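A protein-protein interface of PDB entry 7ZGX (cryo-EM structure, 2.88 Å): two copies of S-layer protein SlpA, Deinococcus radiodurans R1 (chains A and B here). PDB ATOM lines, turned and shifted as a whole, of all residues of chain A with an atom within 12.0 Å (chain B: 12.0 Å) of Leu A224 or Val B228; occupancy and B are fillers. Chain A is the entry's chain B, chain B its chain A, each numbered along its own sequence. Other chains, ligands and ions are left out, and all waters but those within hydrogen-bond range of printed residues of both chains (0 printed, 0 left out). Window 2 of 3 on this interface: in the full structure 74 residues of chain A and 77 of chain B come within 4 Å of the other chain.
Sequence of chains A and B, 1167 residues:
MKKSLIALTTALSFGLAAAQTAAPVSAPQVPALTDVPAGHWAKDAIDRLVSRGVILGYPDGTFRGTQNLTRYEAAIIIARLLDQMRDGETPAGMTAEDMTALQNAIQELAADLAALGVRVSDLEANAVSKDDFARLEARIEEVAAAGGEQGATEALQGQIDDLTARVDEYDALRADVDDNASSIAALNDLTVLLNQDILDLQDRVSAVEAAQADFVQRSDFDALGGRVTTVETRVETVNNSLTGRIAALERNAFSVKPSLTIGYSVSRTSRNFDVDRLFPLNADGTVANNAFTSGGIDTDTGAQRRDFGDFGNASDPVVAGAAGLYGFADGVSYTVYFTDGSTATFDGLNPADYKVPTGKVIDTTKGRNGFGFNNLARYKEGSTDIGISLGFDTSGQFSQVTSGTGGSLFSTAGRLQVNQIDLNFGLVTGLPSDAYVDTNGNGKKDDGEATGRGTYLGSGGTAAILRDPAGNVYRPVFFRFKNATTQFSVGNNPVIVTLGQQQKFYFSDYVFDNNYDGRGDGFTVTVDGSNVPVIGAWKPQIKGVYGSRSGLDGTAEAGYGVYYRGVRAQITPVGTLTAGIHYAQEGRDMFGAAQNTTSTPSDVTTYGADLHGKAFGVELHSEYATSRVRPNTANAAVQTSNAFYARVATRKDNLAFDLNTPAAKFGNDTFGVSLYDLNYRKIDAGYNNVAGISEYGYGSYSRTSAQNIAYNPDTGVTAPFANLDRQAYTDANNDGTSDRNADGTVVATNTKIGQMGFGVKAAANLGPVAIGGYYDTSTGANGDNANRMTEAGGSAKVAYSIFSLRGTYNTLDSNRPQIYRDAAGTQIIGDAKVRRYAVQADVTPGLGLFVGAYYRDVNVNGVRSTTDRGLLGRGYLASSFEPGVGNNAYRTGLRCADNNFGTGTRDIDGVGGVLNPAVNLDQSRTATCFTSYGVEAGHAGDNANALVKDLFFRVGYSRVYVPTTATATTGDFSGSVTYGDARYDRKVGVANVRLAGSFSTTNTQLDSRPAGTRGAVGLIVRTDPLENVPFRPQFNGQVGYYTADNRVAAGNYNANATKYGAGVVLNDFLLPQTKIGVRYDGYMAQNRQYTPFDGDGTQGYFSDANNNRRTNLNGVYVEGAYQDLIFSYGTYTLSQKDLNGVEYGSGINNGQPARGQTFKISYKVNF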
ATOM      1  N   SER A 219      26.816  11.692 -19.109  1.00  0.00           N
ATOM      2  CA  SER A 219      25.538  10.993 -19.133  1.00  0.00           C
ATOM      3  C   SER A 219      24.528  11.741 -19.999  1.00  0.00           C
ATOM      4  O   SER A 219      24.844  12.161 -21.113  1.00  0.00           O
ATOM      5  CB  SER A 219      24.997  10.817 -17.713  1.00  0.00           C
ATOM      6  OG  SER A 219      23.813  10.042 -17.709  1.00  0.00           O
ATOM      7  N   ASP A 220      23.311  11.908 -19.480  1.00  0.00           N
ATOM      8  CA  ASP A 220      22.234  12.573 -20.203  1.00  0.00           C
ATOM      9  C   ASP A 220      21.906  13.959 -19.664  1.00  0.00           C
ATOM     10  O   ASP A 220      20.865  14.517 -20.027  1.00  0.00           O
ATOM     11  CB  ASP A 220      20.974  11.700 -20.194  1.00  0.00           C
ATOM     12  CG  ASP A 220      20.559  11.289 -18.794  1.00  0.00           C
ATOM     13  OD1 ASP A 220      21.304  11.590 -17.839  1.00  0.00           O
ATOM     14  OD2 ASP A 220      19.487  10.667 -18.648  1.00  0.00           O
ATOM     15  N   PHE A 221      22.749  14.524 -18.800  1.00  0.00           N
ATOM     16  CA  PHE A 221      22.593  15.921 -18.399  1.00  0.00           C
ATOM     17  C   PHE A 221      23.477  16.879 -19.177  1.00  0.00           C
ATOM     18  O   PHE A 221      23.542  18.039 -18.760  1.00  0.00           O
ATOM     19  CB  PHE A 221      22.845  16.099 -16.901  1.00  0.00           C
ATOM     20  CG  PHE A 221      21.688  15.691 -16.036  1.00  0.00           C
ATOM     21  CD1 PHE A 221      20.434  15.491 -16.587  1.00  0.00           C
ATOM     22  CD2 PHE A 221      21.837  15.565 -14.668  1.00  0.00           C
ATOM     23  CE1 PHE A 221      19.362  15.139 -15.791  1.00  0.00           C
ATOM     24  CE2 PHE A 221      20.767  15.213 -13.870  1.00  0.00           C
ATOM     25  CZ  PHE A 221      19.530  15.002 -14.431  1.00  0.00           C
ATOM     26  N   ASP A 222      24.169  16.510 -20.255  1.00  0.00           N
ATOM     27  CA  ASP A 222      24.833  17.528 -21.061  1.00  0.00           C
ATOM     28  C   ASP A 222      23.836  18.456 -21.743  1.00  0.00           C
ATOM     29  O   ASP A 222      24.146  19.636 -21.947  1.00  0.00           O
ATOM     30  CB  ASP A 222      25.746  16.875 -22.095  1.00  0.00           C
ATOM     31  CG  ASP A 222      26.958  16.229 -21.465  1.00  0.00           C
ATOM     32  OD1 ASP A 222      27.392  16.712 -20.399  1.00  0.00           O
ATOM     33  OD2 ASP A 222      27.479  15.246 -22.033  1.00  0.00           O
ATOM     34  N   ALA A 223      22.650  17.955 -22.094  1.00  0.00           N
ATOM     35  CA  ALA A 223      21.598  18.842 -22.576  1.00  0.00           C
ATOM     36  C   ALA A 223      21.237  19.873 -21.517  1.00  0.00           C
ATOM     37  O   ALA A 223      20.982  21.042 -21.835  1.00  0.00           O
ATOM     38  CB  ALA A 223      20.368  18.030 -22.981  1.00  0.00           C
ATOM     39  N   LEU A 224      21.215  19.456 -20.251  1.00  0.00           N
ATOM     40  CA  LEU A 224      21.021  20.406 -19.165  1.00  0.00           C
ATOM     41  C   LEU A 224      22.167  21.407 -19.116  1.00  0.00           C
ATOM     42  O   LEU A 224      21.956  22.595 -18.844  1.00  0.00           O
ATOM     43  CB  LEU A 224      20.899  19.658 -17.842  1.00  0.00           C
ATOM     44  CG  LEU A 224      20.350  20.451 -16.665  1.00  0.00           C
ATOM     45  CD1 LEU A 224      18.946  20.875 -16.998  1.00  0.00           C
ATOM     46  CD2 LEU A 224      20.358  19.605 -15.415  1.00  0.00           C
ATOM     47  N   GLY A 225      23.389  20.943 -19.385  1.00  0.00           N
ATOM     48  CA  GLY A 225      24.532  21.835 -19.438  1.00  0.00           C
ATOM     49  C   GLY A 225      24.490  22.816 -20.588  1.00  0.00           C
ATOM     50  O   GLY A 225      25.166  23.848 -20.533  1.00  0.00           O
ATOM     51  N   GLY A 226      23.728  22.512 -21.633  1.00  0.00           N
ATOM     52  CA  GLY A 226      23.540  23.456 -22.717  1.00  0.00           C
ATOM     53  C   GLY A 226      22.431  24.442 -22.417  1.00  0.00           C
ATOM     54  O   GLY A 226      22.528  25.633 -22.736  1.00  0.00           O
ATOM     55  N   ARG A 227      21.360  23.942 -21.798  1.00  0.00           N
ATOM     56  CA  ARG A 227      20.258  24.812 -21.406  1.00  0.00           C
ATOM     57  C   ARG A 227      20.695  25.843 -20.374  1.00  0.00           C
ATOM     58  O   ARG A 227      20.295  27.011 -20.455  1.00  0.00           O
ATOM     59  CB  ARG A 227      19.097  23.974 -20.873  1.00  0.00           C
ATOM     60  CG  ARG A 227      18.473  23.087 -21.932  1.00  0.00           C
ATOM     61  CD  ARG A 227      17.408  22.170 -21.364  1.00  0.00           C
ATOM     62  NE  ARG A 227      16.236  22.902 -20.903  1.00  0.00           N
ATOM     63  CZ  ARG A 227      15.841  22.961 -19.640  1.00  0.00           C
ATOM     64  NH1 ARG A 227      16.495  22.326 -18.682  1.00  0.00           N
ATOM     65  NH2 ARG A 227      14.759  23.669 -19.330  1.00  0.00           N
ATOM     66  N   VAL A 228      21.517  25.440 -19.403  1.00  0.00           N
ATOM     67  CA  VAL A 228      21.982  26.407 -18.416  1.00  0.00           C
ATOM     68  C   VAL A 228      22.823  27.490 -19.076  1.00  0.00           C
ATOM     69  O   VAL A 228      22.719  28.665 -18.714  1.00  0.00           O
ATOM     70  CB  VAL A 228      22.746  25.707 -17.281  1.00  0.00           C
ATOM     71  CG1 VAL A 228      23.931  24.963 -17.824  1.00  0.00           C
ATOM     72  CG2 VAL A 228      23.196  26.722 -16.254  1.00  0.00           C
ATOM     73  N   THR A 229      23.646  27.133 -20.063  1.00  0.00           N
ATOM     74  CA  THR A 229      24.468  28.141 -20.726  1.00  0.00           C
ATOM     75  C   THR A 229      23.620  29.078 -21.576  1.00  0.00           C
ATOM     76  O   THR A 229      23.862  30.294 -21.606  1.00  0.00           O
ATOM     77  CB  THR A 229      25.540  27.467 -21.579  1.00  0.00           C
ATOM     78  OG1 THR A 229      26.326  26.599 -20.754  1.00  0.00           O
ATOM     79  CG2 THR A 229      26.446  28.507 -22.212  1.00  0.00           C
ATOM     80  N   THR A 230      22.619  28.540 -22.276  1.00  0.00           N
ATOM     81  CA  THR A 230      21.771  29.407 -23.084  1.00  0.00           C
ATOM     82  C   THR A 230      20.977  30.359 -22.196  1.00  0.00           C
ATOM     83  O   THR A 230      20.757  31.517 -22.555  1.00  0.00           O
ATOM     84  CB  THR A 230      20.856  28.587 -23.999  1.00  0.00           C
ATOM     85  OG1 THR A 230      20.367  29.427 -25.050  1.00  0.00           O
ATOM     86  CG2 THR A 230      19.666  28.021 -23.252  1.00  0.00           C
ATOM     87  N   VAL A 231      20.588  29.910 -20.999  1.00  0.00           N
ATOM     88  CA  VAL A 231      19.944  30.829 -20.063  1.00  0.00           C
ATOM     89  C   VAL A 231      20.941  31.850 -19.524  1.00  0.00           C
ATOM     90  O   VAL A 231      20.599  33.023 -19.326  1.00  0.00           O
ATOM     91  CB  VAL A 231      19.271  30.044 -18.925  1.00  0.00           C
ATOM     92  CG1 VAL A 231      19.060  30.928 -17.716  1.00  0.00           C
ATOM     93  CG2 VAL A 231      17.953  29.490 -19.395  1.00  0.00           C
ATOM     94  N   GLU A 232      22.178  31.425 -19.268  1.00  0.00           N
ATOM     95  CA  GLU A 232      23.184  32.319 -18.705  1.00  0.00           C
ATOM     96  C   GLU A 232      23.552  33.427 -19.684  1.00  0.00           C
ATOM     97  O   GLU A 232      23.981  34.513 -19.280  1.00  0.00           O
ATOM     98  CB  GLU A 232      24.415  31.508 -18.301  1.00  0.00           C
ATOM     99  CG  GLU A 232      25.507  32.302 -17.617  1.00  0.00           C
ATOM    100  CD  GLU A 232      26.657  31.424 -17.168  1.00  0.00           C
ATOM    101  OE1 GLU A 232      26.593  30.200 -17.402  1.00  0.00           O
ATOM    102  OE2 GLU A 232      27.624  31.957 -16.585  1.00  0.00           O
ATOM    103  N   THR A 233      23.416  33.161 -20.984  1.00  0.00           N
ATOM    104  CA  THR A 233      23.597  34.241 -21.952  1.00  0.00           C
ATOM    105  C   THR A 233      22.286  34.975 -22.229  1.00  0.00           C
ATOM    106  O   THR A 233      22.303  36.155 -22.604  1.00  0.00           O
ATOM    107  CB  THR A 233      24.198  33.713 -23.252  1.00  0.00           C
ATOM    108  OG1 THR A 233      24.526  34.815 -24.103  1.00  0.00           O
ATOM    109  CG2 THR A 233      23.223  32.811 -23.973  1.00  0.00           C
ATOM    110  N   ARG A 234      21.147  34.306 -22.034  1.00  0.00           N
ATOM    111  CA  ARG A 234      19.859  34.959 -22.218  1.00  0.00           C
ATOM    112  C   ARG A 234      19.642  36.055 -21.187  1.00  0.00           C
ATOM    113  O   ARG A 234      19.080  37.106 -21.502  1.00  0.00           O
ATOM    114  CB  ARG A 234      18.740  33.926 -22.142  1.00  0.00           C
ATOM    115  CG  ARG A 234      17.351  34.517 -22.155  1.00  0.00           C
ATOM    116  CD  ARG A 234      17.059  35.178 -23.482  1.00  0.00           C
ATOM    117  NE  ARG A 234      15.640  35.467 -23.635  1.00  0.00           N
ATOM    118  CZ  ARG A 234      15.160  36.561 -24.206  1.00  0.00           C
ATOM    119  NH1 ARG A 234      15.960  37.493 -24.695  1.00  0.00           N
ATOM    120  NH2 ARG A 234      13.843  36.722 -24.294  1.00  0.00           N
ATOM    121  N   VAL A 235      20.065  35.826 -19.946  1.00  0.00           N
ATOM    122  CA  VAL A 235      19.902  36.858 -18.923  1.00  0.00           C
ATOM    123  C   VAL A 235      20.712  38.095 -19.293  1.00  0.00           C
ATOM    124  O   VAL A 235      20.248  39.233 -19.149  1.00  0.00           O
ATOM    125  CB  VAL A 235      20.276  36.316 -17.533  1.00  0.00           C
ATOM    126  CG1 VAL A 235      21.710  35.834 -17.497  1.00  0.00           C
ATOM    127  CG2 VAL A 235      20.061  37.383 -16.487  1.00  0.00           C
ATOM    128  N   SER B 219      20.653  10.522 -10.377  1.00  0.00           N
ATOM    129  CA  SER B 219      20.827  10.767  -8.952  1.00  0.00           C
ATOM    130  C   SER B 219      19.878  11.865  -8.479  1.00  0.00           C
ATOM    131  O   SER B 219      18.693  11.856  -8.813  1.00  0.00           O
ATOM    132  CB  SER B 219      22.277  11.143  -8.645  1.00  0.00           C
ATOM    133  OG  SER B 219      22.489  11.283  -7.251  1.00  0.00           O
ATOM    134  N   ASP B 220      20.404  12.810  -7.699  1.00  0.00           N
ATOM    135  CA  ASP B 220      19.611  13.914  -7.172  1.00  0.00           C
ATOM    136  C   ASP B 220      19.811  15.213  -7.937  1.00  0.00           C
ATOM    137  O   ASP B 220      19.516  16.283  -7.397  1.00  0.00           O
ATOM    138  CB  ASP B 220      19.925  14.146  -5.689  1.00  0.00           C
ATOM    139  CG  ASP B 220      21.389  14.444  -5.440  1.00  0.00           C
ATOM    140  OD1 ASP B 220      22.188  14.375  -6.396  1.00  0.00           O
ATOM    141  OD2 ASP B 220      21.739  14.752  -4.281  1.00  0.00           O
ATOM    142  N   PHE B 221      20.320  15.156  -9.155  1.00  0.00           N
ATOM    143  CA  PHE B 221      20.388  16.391  -9.918  1.00  0.00           C
ATOM    144  C   PHE B 221      19.129  16.644 -10.722  1.00  0.00           C
ATOM    145  O   PHE B 221      19.103  17.586 -11.518  1.00  0.00           O
ATOM    146  CB  PHE B 221      21.613  16.390 -10.833  1.00  0.00           C
ATOM    147  CG  PHE B 221      22.862  16.921 -10.177  1.00  0.00           C
ATOM    148  CD1 PHE B 221      24.012  17.136 -10.917  1.00  0.00           C
ATOM    149  CD2 PHE B 221      22.885  17.201  -8.822  1.00  0.00           C
ATOM    150  CE1 PHE B 221      25.157  17.623 -10.317  1.00  0.00           C
ATOM    151  CE2 PHE B 221      24.030  17.686  -8.220  1.00  0.00           C
ATOM    152  CZ  PHE B 221      25.167  17.898  -8.972  1.00  0.00           C
ATOM    153  N   ASP B 222      18.078  15.838 -10.563  1.00  0.00           N
ATOM    154  CA  ASP B 222      16.788  16.194 -11.139  1.00  0.00           C
ATOM    155  C   ASP B 222      16.193  17.429 -10.477  1.00  0.00           C
ATOM    156  O   ASP B 222      15.561  18.241 -11.162  1.00  0.00           O
ATOM    157  CB  ASP B 222      15.814  15.021 -11.031  1.00  0.00           C
ATOM    158  CG  ASP B 222      16.344  13.763 -11.687  1.00  0.00           C
ATOM    159  OD1 ASP B 222      17.183  13.076 -11.068  1.00  0.00           O
ATOM    160  OD2 ASP B 222      15.924  13.464 -12.824  1.00  0.00           O
ATOM    161  N   ALA B 223      16.374  17.582  -9.163  1.00  0.00           N
ATOM    162  CA  ALA B 223      15.983  18.824  -8.506  1.00  0.00           C
ATOM    163  C   ALA B 223      16.693  20.016  -9.135  1.00  0.00           C
ATOM    164  O   ALA B 223      16.109  21.097  -9.273  1.00  0.00           O
ATOM    165  CB  ALA B 223      16.284  18.743  -7.010  1.00  0.00           C
ATOM    166  N   LEU B 224      17.952  19.830  -9.531  1.00  0.00           N
ATOM    167  CA  LEU B 224      18.652  20.865 -10.280  1.00  0.00           C
ATOM    168  C   LEU B 224      17.967  21.124 -11.614  1.00  0.00           C
ATOM    169  O   LEU B 224      17.872  22.273 -12.064  1.00  0.00           O
ATOM    170  CB  LEU B 224      20.108  20.452 -10.482  1.00  0.00           C
ATOM    171  CG  LEU B 224      21.107  21.476 -11.003  1.00  0.00           C
ATOM    172  CD1 LEU B 224      22.456  21.187 -10.399  1.00  0.00           C
ATOM    173  CD2 LEU B 224      21.195  21.423 -12.507  1.00  0.00           C
ATOM    174  N   GLY B 225      17.483  20.064 -12.263  1.00  0.00           N
ATOM    175  CA  GLY B 225      16.741  20.224 -13.499  1.00  0.00           C
ATOM    176  C   GLY B 225      15.407  20.915 -13.324  1.00  0.00           C
ATOM    177  O   GLY B 225      14.854  21.432 -14.298  1.00  0.00           O
ATOM    178  N   GLY B 226      14.869  20.915 -12.110  1.00  0.00           N
ATOM    179  CA  GLY B 226      13.670  21.680 -11.837  1.00  0.00           C
ATOM    180  C   GLY B 226      13.996  23.132 -11.559  1.00  0.00           C
ATOM    181  O   GLY B 226      13.283  24.043 -11.997  1.00  0.00           O
ATOM    182  N   ARG B 227      15.090  23.352 -10.828  1.00  0.00           N
ATOM    183  CA  ARG B 227      15.527  24.713 -10.540  1.00  0.00           C
ATOM    184  C   ARG B 227      15.886  25.462 -11.815  1.00  0.00           C
ATOM    185  O   ARG B 227      15.574  26.653 -11.949  1.00  0.00           O
ATOM    186  CB  ARG B 227      16.718  24.689  -9.585  1.00  0.00           C
ATOM    187  CG  ARG B 227      16.398  24.099  -8.225  1.00  0.00           C
ATOM    188  CD  ARG B 227      17.653  23.892  -7.395  1.00  0.00           C
ATOM    189  NE  ARG B 227      18.261  25.155  -6.997  1.00  0.00           N
ATOM    190  CZ  ARG B 227      19.392  25.630  -7.496  1.00  0.00           C
ATOM    191  NH1 ARG B 227      20.067  24.974  -8.425  1.00  0.00           N
ATOM    192  NH2 ARG B 227      19.857  26.794  -7.052  1.00  0.00           N
ATOM    193  N   VAL B 228      16.529  24.784 -12.765  1.00  0.00           N
ATOM    194  CA  VAL B 228      16.853  25.454 -14.017  1.00  0.00           C
ATOM    195  C   VAL B 228      15.584  25.813 -14.776  1.00  0.00           C
ATOM    196  O   VAL B 228      15.518  26.865 -15.411  1.00  0.00           O
ATOM    197  CB  VAL B 228      17.806  24.596 -14.868  1.00  0.00           C
ATOM    198  CG1 VAL B 228      17.130  23.328 -15.306  1.00  0.00           C
ATOM    199  CG2 VAL B 228      18.299  25.382 -16.067  1.00  0.00           C
ATOM    200  N   THR B 229      14.551  24.969 -14.715  1.00  0.00           N
ATOM    201  CA  THR B 229      13.288  25.301 -15.368  1.00  0.00           C
ATOM    202  C   THR B 229      12.618  26.499 -14.702  1.00  0.00           C
ATOM    203  O   THR B 229      12.019  27.348 -15.378  1.00  0.00           O
ATOM    204  CB  THR B 229      12.359  24.088 -15.354  1.00  0.00           C
ATOM    205  OG1 THR B 229      12.992  22.995 -16.029  1.00  0.00           O
ATOM    206  CG2 THR B 229      11.050  24.407 -16.049  1.00  0.00           C
ATOM    207  N   THR B 230      12.702  26.580 -13.372  1.00  0.00           N
ATOM    208  CA  THR B 230      12.200  27.767 -12.685  1.00  0.00           C
ATOM    209  C   THR B 230      12.944  29.011 -13.151  1.00  0.00           C
ATOM    210  O   THR B 230      12.341  30.069 -13.342  1.00  0.00           O
ATOM    211  CB  THR B 230      12.315  27.614 -11.167  1.00  0.00           C
ATOM    212  OG1 THR B 230      13.693  27.634 -10.779  1.00  0.00           O
ATOM    213  CG2 THR B 230      11.660  26.330 -10.699  1.00  0.00           C
ATOM    214  N   VAL B 231      14.259  28.902 -13.344  1.00  0.00           N
ATOM    215  CA  VAL B 231      15.003  30.033 -13.898  1.00  0.00           C
ATOM    216  C   VAL B 231      14.538  30.345 -15.316  1.00  0.00           C
ATOM    217  O   VAL B 231      14.448  31.516 -15.709  1.00  0.00           O
ATOM    218  CB  VAL B 231      16.515  29.757 -13.859  1.00  0.00           C
ATOM    219  CG1 VAL B 231      17.270  30.888 -14.525  1.00  0.00           C
ATOM    220  CG2 VAL B 231      16.984  29.582 -12.429  1.00  0.00           C
ATOM    221  N   GLU B 232      14.239  29.309 -16.100  1.00  0.00           N
ATOM    222  CA  GLU B 232      13.810  29.486 -17.482  1.00  0.00           C
ATOM    223  C   GLU B 232      12.522  30.294 -17.551  1.00  0.00           C
ATOM    224  O   GLU B 232      12.364  31.176 -18.400  1.00  0.00           O
ATOM    225  CB  GLU B 232      13.610  28.120 -18.141  1.00  0.00           C
ATOM    226  CG  GLU B 232      14.880  27.322 -18.360  1.00  0.00           C
ATOM    227  CD  GLU B 232      15.383  27.399 -19.777  1.00  0.00           C
ATOM    228  OE1 GLU B 232      16.176  26.522 -20.173  1.00  0.00           O
ATOM    229  OE2 GLU B 232      14.993  28.343 -20.494  1.00  0.00           O
ATOM    230  N   THR B 233      11.575  29.983 -16.667  1.00  0.00           N
ATOM    231  CA  THR B 233      10.333  30.752 -16.649  1.00  0.00           C
ATOM    232  C   THR B 233      10.518  32.109 -15.975  1.00  0.00           C
ATOM    233  O   THR B 233       9.838  33.077 -16.339  1.00  0.00           O
ATOM    234  CB  THR B 233       9.212  29.960 -15.972  1.00  0.00           C
ATOM    235  OG1 THR B 233       7.976  30.668 -16.113  1.00  0.00           O
ATOM    236  CG2 THR B 233       9.493  29.755 -14.498  1.00  0.00           C
ATOM    237  N   ARG B 234      11.435  32.209 -15.010  1.00  0.00           N
ATOM    238  CA  ARG B 234      11.638  33.470 -14.313  1.00  0.00           C
ATOM    239  C   ARG B 234      12.228  34.523 -15.232  1.00  0.00           C
ATOM    240  O   ARG B 234      11.815  35.685 -15.195  1.00  0.00           O
ATOM    241  CB  ARG B 234      12.542  33.264 -13.102  1.00  0.00           C
ATOM    242  CG  ARG B 234      12.914  34.551 -12.400  1.00  0.00           C
ATOM    243  CD  ARG B 234      11.701  35.181 -11.752  1.00  0.00           C
ATOM    244  NE  ARG B 234      12.068  36.268 -10.854  1.00  0.00           N
ATOM    245  CZ  ARG B 234      11.341  37.360 -10.668  1.00  0.00           C
ATOM    246  NH1 ARG B 234      10.194  37.541 -11.300  1.00  0.00           N
ATOM    247  NH2 ARG B 234      11.773  38.291  -9.822  1.00  0.00           N
ATOM    248  N   VAL B 235      13.204  34.148 -16.059  1.00  0.00           N
ATOM    249  CA  VAL B 235      13.826  35.136 -16.937  1.00  0.00           C
ATOM    250  C   VAL B 235      12.803  35.660 -17.939  1.00  0.00           C
ATOM    251  O   VAL B 235      12.766  36.855 -18.256  1.00  0.00           O
ATOM    252  CB  VAL B 235      15.069  34.546 -17.629  1.00  0.00           C
ATOM    253  CG1 VAL B 235      14.690  33.477 -18.636  1.00  0.00           C
ATOM    254  CG2 VAL B 235      15.877  35.644 -18.289  1.00  0.00           C
ATOM    255  N   GLU B 236      11.913  34.783 -18.401  1.00  0.00           N
ATOM    256  CA  GLU B 236      10.906  35.202 -19.367  1.00  0.00           C
ATOM    257  C   GLU B 236       9.847  36.083 -18.720  1.00  0.00           C
ATOM    258  O   GLU B 236       9.428  37.085 -19.306  1.00  0.00           O
ATOM    259  CB  GLU B 236      10.273  33.983 -20.029  1.00  0.00           C
ATOM    260  CG  GLU B 236      11.169  33.365 -21.073  1.00  0.00           C
ATOM    261  CD  GLU B 236      11.969  34.411 -21.818  1.00  0.00           C
ATOM    262  OE1 GLU B 236      11.375  35.138 -22.637  1.00  0.00           O
ATOM    263  OE2 GLU B 236      13.188  34.513 -21.579  1.00  0.00           O
ATOM    264  N   THR B 237       9.396  35.735 -17.514  1.00  0.00           N
ATOM    265  CA  THR B 237       8.419  36.597 -16.861  1.00  0.00           C
ATOM    266  C   THR B 237       9.031  37.950 -16.516  1.00  0.00           C
ATOM    267  O   THR B 237       8.358  38.980 -16.606  1.00  0.00           O
ATOM    268  CB  THR B 237       7.823  35.926 -15.619  1.00  0.00           C
ATOM    269  OG1 THR B 237       6.740  36.723 -15.124  1.00  0.00           O
ATOM    270  CG2 THR B 237       8.841  35.766 -14.518  1.00  0.00           C
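Of chain B, only Leu B224 and Val B228 come within 4 Å of Leu A224. Printed residues of chain A within 4 Å of Val B228: Leu A224 (3.5 Å) and Arg A227 (3.6 Å). Phe A221 touches just one residue of chain B: Phe B221. No residue of chain B comes within 4 Å of Asp A222. No residue of chain B comes within 4 Å of Gly A225. No residue of chain B comes within 4 Å of Gly A226. Val A228 touches none of the printed residues of chain B. Leu B224 touches just one residue of chain A: Leu A224 (3.5 Å). No residue of chain A comes within 4 Å of Gly B225. No residue of chain A comes within 4 Å of Arg B227. Of chain A, only Arg A227 (3.8 Å) comes within 4 Å of Thr B229. No residue of chain A comes within 4 Å of Thr B230. Of chain A, only Arg A227 and Val A231 come within 4 Å of Glu B232. Of the printed residues of chain A, Glu B236 touches Arg A234 (3.3 Å). Of the printed residues of chain B, Val A231 touches Val B231 (3.7 Å) and Glu B232 (3.3 Å). Printed residues of chain B within 4 Å of Arg A234: Glu B236 (3.3 Å). Asp A220 touches none of the printed residues of chain B. The nearest residue of chain B that does not touch Leu A224 is Gly B225 (4.1 Å). The nearest residue of chain A that does not touch Val B228 is Val A228 (4.5 Å).
Among the printed residues, merely in contact across the chains: Val A231 with Glu B232, Phe A221 with Phe B221, Leu A224 with Val B228, Leu A224 with Leu B224, Arg A227 with Val B228, Val A231 with Val B231 and Arg A227 with Thr B229.
Phe B221 touches its own counterpart, Phe A221. Leu A224 touches its own counterpart, Leu B224. Arg A227 touches Val B228, but with the chains exchanged Val A228 does not touch Arg B227 (8.6 Å). Arg A227 touches Glu B232, but with the chains exchanged Glu A232 does not touch Arg B227 (11.0 Å). Positions printed for both chains: 219, 220, 221, 222, 223, 224, 225, 226, 227, 228, 229, 230, 231, 232, 233, 234 and 235.
Of the 17 printed residues of chain A, 5 touch a printed residue of chain B. Hydrophobic or aromatic side chains of chain A within 4 Å of the printed part of chain B: Phe A221, Leu A224 and Val A231. Of the 19 printed residues of chain B, 7 touch a printed residue of chain A. Hydrophobic or aromatic side chains of chain B that line the printed part of chain A: Phe B221, Leu B224, Val B228 and Val B231. Among the printed residues, 9 pairs touch across the chains. Among the printed residues, Asp or Glu carboxylates within 4 Å of a Lys or Arg side-chain nitrogen of the other chain: Arg A227 with Glu B232 and Arg A234 with Glu B236.
O of Gly B225 is in hydrogen-bond range of OG1 of Thr B229.
NH2 of Arg A227 lies within salt-bridge range of OE1 of Glu B232 (3.3 Å). The side-chain carboxylate (OE2) of Glu B236 lies within salt-bridge range of the guanidinium group (NE) of Arg A234 (3.3 Å).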
